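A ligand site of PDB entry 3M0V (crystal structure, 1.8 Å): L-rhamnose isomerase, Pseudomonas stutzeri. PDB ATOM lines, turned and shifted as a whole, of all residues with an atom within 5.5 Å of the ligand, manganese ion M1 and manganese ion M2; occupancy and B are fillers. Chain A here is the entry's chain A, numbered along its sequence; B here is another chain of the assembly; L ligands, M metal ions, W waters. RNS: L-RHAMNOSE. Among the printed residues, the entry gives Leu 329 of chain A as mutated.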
ATOM      1  N   TRP A  57      18.584  -0.855  18.473  1.00  0.00           N
ATOM      2  CA  TRP A  57      18.808  -2.282  18.257  1.00  0.00           C
ATOM      3  C   TRP A  57      19.790  -2.602  17.127  1.00  0.00           C
ATOM      4  O   TRP A  57      20.113  -3.770  16.889  1.00  0.00           O
ATOM      5  CB  TRP A  57      17.472  -2.990  18.034  1.00  0.00           C
ATOM      6  CG  TRP A  57      16.713  -2.538  16.824  1.00  0.00           C
ATOM      7  CD1 TRP A  57      16.766  -3.096  15.579  1.00  0.00           C
ATOM      8  CD2 TRP A  57      15.787  -1.450  16.746  1.00  0.00           C
ATOM      9  NE1 TRP A  57      15.915  -2.427  14.726  1.00  0.00           N
ATOM     10  CE2 TRP A  57      15.299  -1.411  15.418  1.00  0.00           C
ATOM     11  CE3 TRP A  57      15.308  -0.511  17.671  1.00  0.00           C
ATOM     12  CZ2 TRP A  57      14.361  -0.464  14.991  1.00  0.00           C
ATOM     13  CZ3 TRP A  57      14.376   0.434  17.237  1.00  0.00           C
ATOM     14  CH2 TRP A  57      13.919   0.451  15.914  1.00  0.00           C
ATOM     15  N   HIS A 101      13.505   0.856  21.816  1.00  0.00           N
ATOM     16  CA  HIS A 101      12.675  -0.337  21.710  1.00  0.00           C
ATOM     17  C   HIS A 101      12.438  -0.861  23.128  1.00  0.00           C
ATOM     18  O   HIS A 101      13.386  -1.093  23.880  1.00  0.00           O
ATOM     19  CB  HIS A 101      13.374  -1.389  20.856  1.00  0.00           C
ATOM     20  CG  HIS A 101      12.452  -2.196  19.999  1.00  0.00           C
ATOM     21  ND1 HIS A 101      11.480  -3.019  20.523  1.00  0.00           N
ATOM     22  CD2 HIS A 101      12.342  -2.298  18.656  1.00  0.00           C
ATOM     23  CE1 HIS A 101      10.826  -3.606  19.534  1.00  0.00           C
ATOM     24  NE2 HIS A 101      11.327  -3.180  18.389  1.00  0.00           N
ATOM     25  N   TRP A 104      13.543  -3.919  25.482  1.00  0.00           N
ATOM     26  CA  TRP A 104      15.000  -3.981  25.350  1.00  0.00           C
ATOM     27  C   TRP A 104      15.700  -2.799  25.993  1.00  0.00           C
ATOM     28  O   TRP A 104      16.678  -2.967  26.727  1.00  0.00           O
ATOM     29  CB  TRP A 104      15.433  -4.074  23.883  1.00  0.00           C
ATOM     30  CG  TRP A 104      14.973  -5.310  23.158  1.00  0.00           C
ATOM     31  CD1 TRP A 104      14.640  -6.516  23.714  1.00  0.00           C
ATOM     32  CD2 TRP A 104      14.804  -5.461  21.746  1.00  0.00           C
ATOM     33  NE1 TRP A 104      14.282  -7.413  22.724  1.00  0.00           N
ATOM     34  CE2 TRP A 104      14.378  -6.786  21.509  1.00  0.00           C
ATOM     35  CE3 TRP A 104      14.982  -4.599  20.653  1.00  0.00           C
ATOM     36  CZ2 TRP A 104      14.107  -7.270  20.221  1.00  0.00           C
ATOM     37  CZ3 TRP A 104      14.721  -5.084  19.375  1.00  0.00           C
ATOM     38  CH2 TRP A 104      14.292  -6.399  19.174  1.00  0.00           C
ATOM     39  N   ASN A 127       9.204   2.135  20.021  1.00  0.00           N
ATOM     40  CA  ASN A 127       8.854   0.876  19.363  1.00  0.00           C
ATOM     41  C   ASN A 127       8.437  -0.113  20.422  1.00  0.00           C
ATOM     42  O   ASN A 127       9.178  -0.350  21.373  1.00  0.00           O
ATOM     43  CB  ASN A 127      10.057   0.314  18.604  1.00  0.00           C
ATOM     44  CG  ASN A 127      10.472   1.197  17.447  1.00  0.00           C
ATOM     45  OD1 ASN A 127       9.992   1.041  16.319  1.00  0.00           O
ATOM     46  ND2 ASN A 127      11.373   2.127  17.707  1.00  0.00           N
ATOM     47  N   SER A 128       7.246  -0.684  20.268  1.00  0.00           N
ATOM     48  CA  SER A 128       6.732  -1.680  21.210  1.00  0.00           C
ATOM     49  C   SER A 128       7.210  -3.062  20.785  1.00  0.00           C
ATOM     50  O   SER A 128       7.584  -3.276  19.631  1.00  0.00           O
ATOM     51  CB  SER A 128       5.209  -1.645  21.232  1.00  0.00           C
ATOM     52  OG  SER A 128       4.663  -1.867  19.935  1.00  0.00           O
ATOM     53  N   PHE A 131       6.291  -9.289  19.978  1.00  0.00           N
ATOM     54  CA  PHE A 131       6.637 -10.350  19.034  1.00  0.00           C
ATOM     55  C   PHE A 131       7.596 -11.316  19.721  1.00  0.00           C
ATOM     56  O   PHE A 131       8.181 -12.204  19.105  1.00  0.00           O
ATOM     57  CB  PHE A 131       7.260  -9.772  17.751  1.00  0.00           C
ATOM     58  CG  PHE A 131       8.415  -8.823  17.990  1.00  0.00           C
ATOM     59  CD1 PHE A 131       9.681  -9.301  18.312  1.00  0.00           C
ATOM     60  CD2 PHE A 131       8.224  -7.445  17.888  1.00  0.00           C
ATOM     61  CE1 PHE A 131      10.746  -8.428  18.517  1.00  0.00           C
ATOM     62  CE2 PHE A 131       9.279  -6.562  18.095  1.00  0.00           C
ATOM     63  CZ  PHE A 131      10.542  -7.054  18.417  1.00  0.00           C
ATOM     64  N   TRP A 179       4.957  -2.770  15.245  1.00  0.00           N
ATOM     65  CA  TRP A 179       5.209  -3.867  14.308  1.00  0.00           C
ATOM     66  C   TRP A 179       5.030  -5.122  15.146  1.00  0.00           C
ATOM     67  O   TRP A 179       5.651  -5.266  16.197  1.00  0.00           O
ATOM     68  CB  TRP A 179       6.633  -3.872  13.752  1.00  0.00           C
ATOM     69  CG  TRP A 179       6.846  -5.121  12.919  1.00  0.00           C
ATOM     70  CD1 TRP A 179       6.281  -5.392  11.715  1.00  0.00           C
ATOM     71  CD2 TRP A 179       7.543  -6.312  13.313  1.00  0.00           C
ATOM     72  NE1 TRP A 179       6.571  -6.677  11.325  1.00  0.00           N
ATOM     73  CE2 TRP A 179       7.338  -7.269  12.288  1.00  0.00           C
ATOM     74  CE3 TRP A 179       8.309  -6.668  14.432  1.00  0.00           C
ATOM     75  CZ2 TRP A 179       7.879  -8.558  12.355  1.00  0.00           C
ATOM     76  CZ3 TRP A 179       8.852  -7.951  14.487  1.00  0.00           C
ATOM     77  CH2 TRP A 179       8.631  -8.883  13.453  1.00  0.00           C
ATOM     78  N   GLU A 219       3.328  -0.733  10.958  1.00  0.00           N
ATOM     79  CA  GLU A 219       4.293  -1.195   9.950  1.00  0.00           C
ATOM     80  C   GLU A 219       3.911  -2.545   9.329  1.00  0.00           C
ATOM     81  O   GLU A 219       3.857  -3.562  10.022  1.00  0.00           O
ATOM     82  CB  GLU A 219       5.684  -1.269  10.596  1.00  0.00           C
ATOM     83  CG  GLU A 219       6.777  -1.870   9.717  1.00  0.00           C
ATOM     84  CD  GLU A 219       8.127  -1.881  10.406  1.00  0.00           C
ATOM     85  OE1 GLU A 219       8.160  -1.766  11.645  1.00  0.00           O
ATOM     86  OE2 GLU A 219       9.161  -2.035   9.710  1.00  0.00           O
ATOM     87  N   LYS A 221       4.309  -5.907   6.830  1.00  0.00           N
ATOM     88  CA  LYS A 221       5.381  -6.823   6.465  1.00  0.00           C
ATOM     89  C   LYS A 221       4.758  -8.059   5.825  1.00  0.00           C
ATOM     90  O   LYS A 221       3.861  -8.680   6.391  1.00  0.00           O
ATOM     91  CB  LYS A 221       6.183  -7.225   7.701  1.00  0.00           C
ATOM     92  CG  LYS A 221       7.490  -7.904   7.364  1.00  0.00           C
ATOM     93  CD  LYS A 221       8.227  -8.355   8.607  1.00  0.00           C
ATOM     94  CE  LYS A 221       9.632  -8.818   8.260  1.00  0.00           C
ATOM     95  NZ  LYS A 221      10.336  -9.329   9.475  1.00  0.00           N
ATOM     96  N   GLU A 224       7.428 -13.326   7.868  1.00  0.00           N
ATOM     97  CA  GLU A 224       8.462 -13.460   8.896  1.00  0.00           C
ATOM     98  C   GLU A 224       8.147 -12.546  10.077  1.00  0.00           C
ATOM     99  O   GLU A 224       8.184 -11.325   9.939  1.00  0.00           O
ATOM    100  CB  GLU A 224       9.867 -13.132   8.370  1.00  0.00           C
ATOM    101  CG  GLU A 224      10.949 -13.399   9.437  1.00  0.00           C
ATOM    102  CD  GLU A 224      12.278 -12.720   9.133  1.00  0.00           C
ATOM    103  OE1 GLU A 224      12.285 -11.604   8.578  1.00  0.00           O
ATOM    104  OE2 GLU A 224      13.328 -13.305   9.493  1.00  0.00           O
ATOM    105  N   LEU A 252       3.815   3.172   8.246  1.00  0.00           N
ATOM    106  CA  LEU A 252       5.265   3.203   8.179  1.00  0.00           C
ATOM    107  C   LEU A 252       5.704   2.186   7.128  1.00  0.00           C
ATOM    108  O   LEU A 252       5.247   1.042   7.119  1.00  0.00           O
ATOM    109  CB  LEU A 252       5.877   2.868   9.539  1.00  0.00           C
ATOM    110  CG  LEU A 252       7.403   3.026   9.591  1.00  0.00           C
ATOM    111  CD1 LEU A 252       7.820   3.609  10.932  1.00  0.00           C
ATOM    112  CD2 LEU A 252       8.070   1.681   9.346  1.00  0.00           C
ATOM    113  N   ASP A 254       8.735   0.067   5.562  1.00  0.00           N
ATOM    114  CA  ASP A 254      10.082  -0.459   5.763  1.00  0.00           C
ATOM    115  C   ASP A 254      10.444  -1.032   4.392  1.00  0.00           C
ATOM    116  O   ASP A 254       9.783  -1.937   3.903  1.00  0.00           O
ATOM    117  CB  ASP A 254      10.068  -1.582   6.803  1.00  0.00           C
ATOM    118  CG  ASP A 254      11.458  -2.112   7.101  1.00  0.00           C
ATOM    119  OD1 ASP A 254      12.170  -2.454   6.129  1.00  0.00           O
ATOM    120  OD2 ASP A 254      11.832  -2.190   8.293  1.00  0.00           O
ATOM    121  N   HIS A 257      10.233  -4.911   3.408  1.00  0.00           N
ATOM    122  CA  HIS A 257       9.027  -5.667   3.765  1.00  0.00           C
ATOM    123  C   HIS A 257       8.018  -5.908   2.642  1.00  0.00           C
ATOM    124  O   HIS A 257       6.836  -6.122   2.912  1.00  0.00           O
ATOM    125  CB  HIS A 257       8.297  -4.948   4.906  1.00  0.00           C
ATOM    126  CG  HIS A 257       9.034  -4.959   6.209  1.00  0.00           C
ATOM    127  ND1 HIS A 257       8.458  -4.536   7.382  1.00  0.00           N
ATOM    128  CD2 HIS A 257      10.299  -5.343   6.518  1.00  0.00           C
ATOM    129  CE1 HIS A 257       9.332  -4.664   8.371  1.00  0.00           C
ATOM    130  NE2 HIS A 257      10.452  -5.148   7.875  1.00  0.00           N
ATOM    131  N   HIS A 281      11.412   3.179   7.284  1.00  0.00           N
ATOM    132  CA  HIS A 281      12.400   2.366   7.970  1.00  0.00           C
ATOM    133  C   HIS A 281      13.334   2.055   6.808  1.00  0.00           C
ATOM    134  O   HIS A 281      12.999   1.240   5.942  1.00  0.00           O
ATOM    135  CB  HIS A 281      11.810   1.076   8.548  1.00  0.00           C
ATOM    136  CG  HIS A 281      11.443   1.168  10.008  1.00  0.00           C
ATOM    137  ND1 HIS A 281      11.116   0.074  10.761  1.00  0.00           N
ATOM    138  CD2 HIS A 281      11.338   2.245  10.822  1.00  0.00           C
ATOM    139  CE1 HIS A 281      10.811   0.457  11.988  1.00  0.00           C
ATOM    140  NE2 HIS A 281      10.941   1.777  12.047  1.00  0.00           N
ATOM    141  N   ASN A 283      16.698   0.714   4.833  1.00  0.00           N
ATOM    142  CA  ASN A 283      17.625  -0.417   4.811  1.00  0.00           C
ATOM    143  C   ASN A 283      17.650  -0.892   3.364  1.00  0.00           C
ATOM    144  O   ASN A 283      16.914  -0.366   2.532  1.00  0.00           O
ATOM    145  CB  ASN A 283      17.164  -1.557   5.733  1.00  0.00           C
ATOM    146  CG  ASN A 283      15.707  -1.968   5.494  1.00  0.00           C
ATOM    147  OD1 ASN A 283      15.329  -2.393   4.396  1.00  0.00           O
ATOM    148  ND2 ASN A 283      14.893  -1.867   6.535  1.00  0.00           N
ATOM    149  N   ASP A 289      13.676  -9.699   3.946  1.00  0.00           N
ATOM    150  CA  ASP A 289      13.867  -8.544   4.819  1.00  0.00           C
ATOM    151  C   ASP A 289      15.301  -8.642   5.345  1.00  0.00           C
ATOM    152  O   ASP A 289      15.533  -8.883   6.520  1.00  0.00           O
ATOM    153  CB  ASP A 289      12.864  -8.567   5.969  1.00  0.00           C
ATOM    154  CG  ASP A 289      12.974  -7.354   6.863  1.00  0.00           C
ATOM    155  OD1 ASP A 289      13.364  -6.283   6.357  1.00  0.00           O
ATOM    156  OD2 ASP A 289      12.665  -7.473   8.073  1.00  0.00           O
ATOM    157  N   ASP A 291      17.629  -6.448   5.869  1.00  0.00           N
ATOM    158  CA  ASP A 291      18.100  -5.422   6.788  1.00  0.00           C
ATOM    159  C   ASP A 291      19.547  -4.998   6.581  1.00  0.00           C
ATOM    160  O   ASP A 291      20.266  -4.749   7.544  1.00  0.00           O
ATOM    161  CB  ASP A 291      17.896  -5.887   8.234  1.00  0.00           C
ATOM    162  CG  ASP A 291      16.449  -5.810   8.664  1.00  0.00           C
ATOM    163  OD1 ASP A 291      15.817  -4.791   8.335  1.00  0.00           O
ATOM    164  OD2 ASP A 291      15.951  -6.761   9.302  1.00  0.00           O
ATOM    165  N   ASP A 327      16.370   1.154   9.941  1.00  0.00           N
ATOM    166  CA  ASP A 327      16.067  -0.088  10.633  1.00  0.00           C
ATOM    167  C   ASP A 327      16.936  -1.134   9.962  1.00  0.00           C
ATOM    168  O   ASP A 327      16.560  -1.715   8.937  1.00  0.00           O
ATOM    169  CB  ASP A 327      14.603  -0.490  10.525  1.00  0.00           C
ATOM    170  CG  ASP A 327      14.297  -1.770  11.294  1.00  0.00           C
ATOM    171  OD1 ASP A 327      15.207  -2.242  12.021  1.00  0.00           O
ATOM    172  OD2 ASP A 327      13.180  -2.305  11.184  1.00  0.00           O
ATOM    173  N   LEU A 329      20.248  -4.297  10.608  1.00  0.00           N
ATOM    174  CA  LEU A 329      20.950  -5.235  11.481  1.00  0.00           C
ATOM    175  C   LEU A 329      22.311  -5.413  10.845  1.00  0.00           C
ATOM    176  O   LEU A 329      22.428  -5.562   9.629  1.00  0.00           O
ATOM    177  CB  LEU A 329      20.214  -6.578  11.547  1.00  0.00           C
ATOM    178  CG  LEU A 329      18.955  -6.629  12.424  1.00  0.00           C
ATOM    179  CD1 LEU A 329      19.309  -6.187  13.844  1.00  0.00           C
ATOM    180  CD2 LEU A 329      17.879  -5.723  11.854  1.00  0.00           C
ATOM    181  N   ARG B  65      14.495 -15.438  13.990  1.00  0.00           N
ATOM    182  CA  ARG B  65      15.469 -14.515  14.570  1.00  0.00           C
ATOM    183  C   ARG B  65      14.818 -13.567  15.582  1.00  0.00           C
ATOM    184  O   ARG B  65      15.518 -12.937  16.378  1.00  0.00           O
ATOM    185  CB  ARG B  65      16.185 -13.714  13.479  1.00  0.00           C
ATOM    186  CG  ARG B  65      15.253 -12.913  12.570  1.00  0.00           C
ATOM    187  CD  ARG B  65      16.034 -11.973  11.641  1.00  0.00           C
ATOM    188  NE  ARG B  65      15.161 -11.372  10.646  1.00  0.00           N
ATOM    189  CZ  ARG B  65      15.341 -10.165  10.115  1.00  0.00           C
ATOM    190  NH1 ARG B  65      16.373  -9.414  10.462  1.00  0.00           N
ATOM    191  NH2 ARG B  65      14.478  -9.714   9.214  1.00  0.00           N
ATOM    192  N   PHE B  66      13.494 -13.480  15.552  1.00  0.00           N
ATOM    193  CA  PHE B  66      12.762 -12.592  16.451  1.00  0.00           C
ATOM    194  C   PHE B  66      12.400 -13.214  17.806  1.00  0.00           C
ATOM    195  O   PHE B  66      12.346 -12.509  18.814  1.00  0.00           O
ATOM    196  CB  PHE B  66      11.470 -12.107  15.781  1.00  0.00           C
ATOM    197  CG  PHE B  66      11.717 -11.207  14.604  1.00  0.00           C
ATOM    198  CD1 PHE B  66      12.157  -9.902  14.803  1.00  0.00           C
ATOM    199  CD2 PHE B  66      11.546 -11.679  13.307  1.00  0.00           C
ATOM    200  CE1 PHE B  66      12.425  -9.083  13.722  1.00  0.00           C
ATOM    201  CE2 PHE B  66      11.815 -10.867  12.215  1.00  0.00           C
ATOM    202  CZ  PHE B  66      12.248  -9.560  12.421  1.00  0.00           C
HETATM  203  C1  RNS L   1      10.509  -6.246  11.636  1.00  0.00           C
HETATM  204  C2  RNS L   1      10.397  -4.736  11.487  1.00  0.00           C
HETATM  205  C3  RNS L   1      10.474  -4.056  12.847  1.00  0.00           C
HETATM  206  C4  RNS L   1      11.683  -4.514  13.668  1.00  0.00           C
HETATM  207  C5  RNS L   1      11.875  -3.629  14.897  1.00  0.00           C
HETATM  208  C6  RNS L   1      13.078  -4.108  15.691  1.00  0.00           C
HETATM  209  O1  RNS L   1      10.749  -6.935  10.643  1.00  0.00           O
HETATM  210  O2  RNS L   1      11.434  -4.266  10.649  1.00  0.00           O
HETATM  211  O3  RNS L   1      10.526  -2.646  12.656  1.00  0.00           O
HETATM  212  O4  RNS L   1      12.859  -4.460  12.866  1.00  0.00           O
HETATM  213  O5  RNS L   1      10.715  -3.678  15.714  1.00  0.00           O
HETATM  214 MN    MN M   1      11.225  -2.048  10.394  1.00  0.00          MN
HETATM  215 MN    MN M   2      11.899  -5.841   9.234  1.00  0.00          MN
HETATM  216  O   HOH W   1       9.067  -1.572  15.419  1.00  0.00           O
HETATM  217  O   HOH W   2      13.452  -6.248  10.570  1.00  0.00           O
HETATM  218  O   HOH W   3      13.277  -4.866   8.335  1.00  0.00           O
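Water W2 bridges OD2 of Asp 291 (2.8 Å) and O4 of the ligand (3.0 Å).
Water W1 bridges O5 of the ligand and OD1 of Asn 127.
The side-chain amino group (NZ) of Lys 221 sits close to an oxygen (O1) of the ligand (2.7 Å).
A ring nitrogen (NE2) of His 101 sits at hydrogen-bond distance from an oxygen (O5) of the ligand (2.8 Å).
NZ of Lys 221 sits close to OD2 of Asp 289, 3.3 Å away.
O of Asp 289 lies within hydrogen-bond range of NH2 of Arg 65 of chain B.
The side-chain amino group (NZ) of Lys 221 is in salt-bridge range of the side-chain carboxylate (OE1) of Glu 224, 3.1 Å away.
OE2 of Glu 219 sits close to ND1 of His 257 (3.5 Å).
OD1 of Asp 254 lies within hydrogen-bond range of ND2 of Asn 283.
ND2 of Asn 283 lies within hydrogen-bond range of O of Asp 327, at 2.9 Å.
The side-chain carboxylate (OD1) of Asp 327 lies within hydrogen-bond range of the indole nitrogen (NE1) of Trp 57, 2.8 Å away.
Within 4 Å of manganese ion M1: Glu 219, Asp 254, His 257, His 281 and Asp 327.
The nearest printed residue that does not touch manganese ion M1 is Leu 252 (5.0 Å).
Residues that only touch the ligand: Trp 57 (3.4 Å), Trp 179 (3.4 Å) and Phe 66 of chain B (3.5 Å).
Within 4 Å of the ligand: Trp 57, His 101, Trp 179, Glu 219, Lys 221, Asp 254, His 257, His 281, Asp 289, Asp 327 and Phe 66 of chain B.
The nearest printed residue that does not touch the ligand is Phe 131 (4.01 Å).
Lys 221 touches manganese ion M2.
Of the 21 residues printed, 4 come within 4 Å of manganese ion M2.
The nearest printed residue that does not touch manganese ion M2 is Asp 291 (4.2 Å).
Manganese ion M2 is bound by water W3 (1.9 Å), water W2 (2.1 Å), a ring nitrogen (NE2) of His 257 (2.1 Å), an oxygen (O1) of the ligand (2.1 Å), the side-chain carboxylate of Asp 289 (2.1 Å) and an oxygen (O2) of the ligand (2.2 Å).
Manganese ion M2 has six donor atoms within binding distance.
Manganese ion M1 is bound by OD2 of Asp 327, ND1 of His 281, OE2 of Glu 219, OD2 of Asp 254, O2 of the ligand and O3 of the ligand.
Manganese ion M1 has six donor atoms within binding distance.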
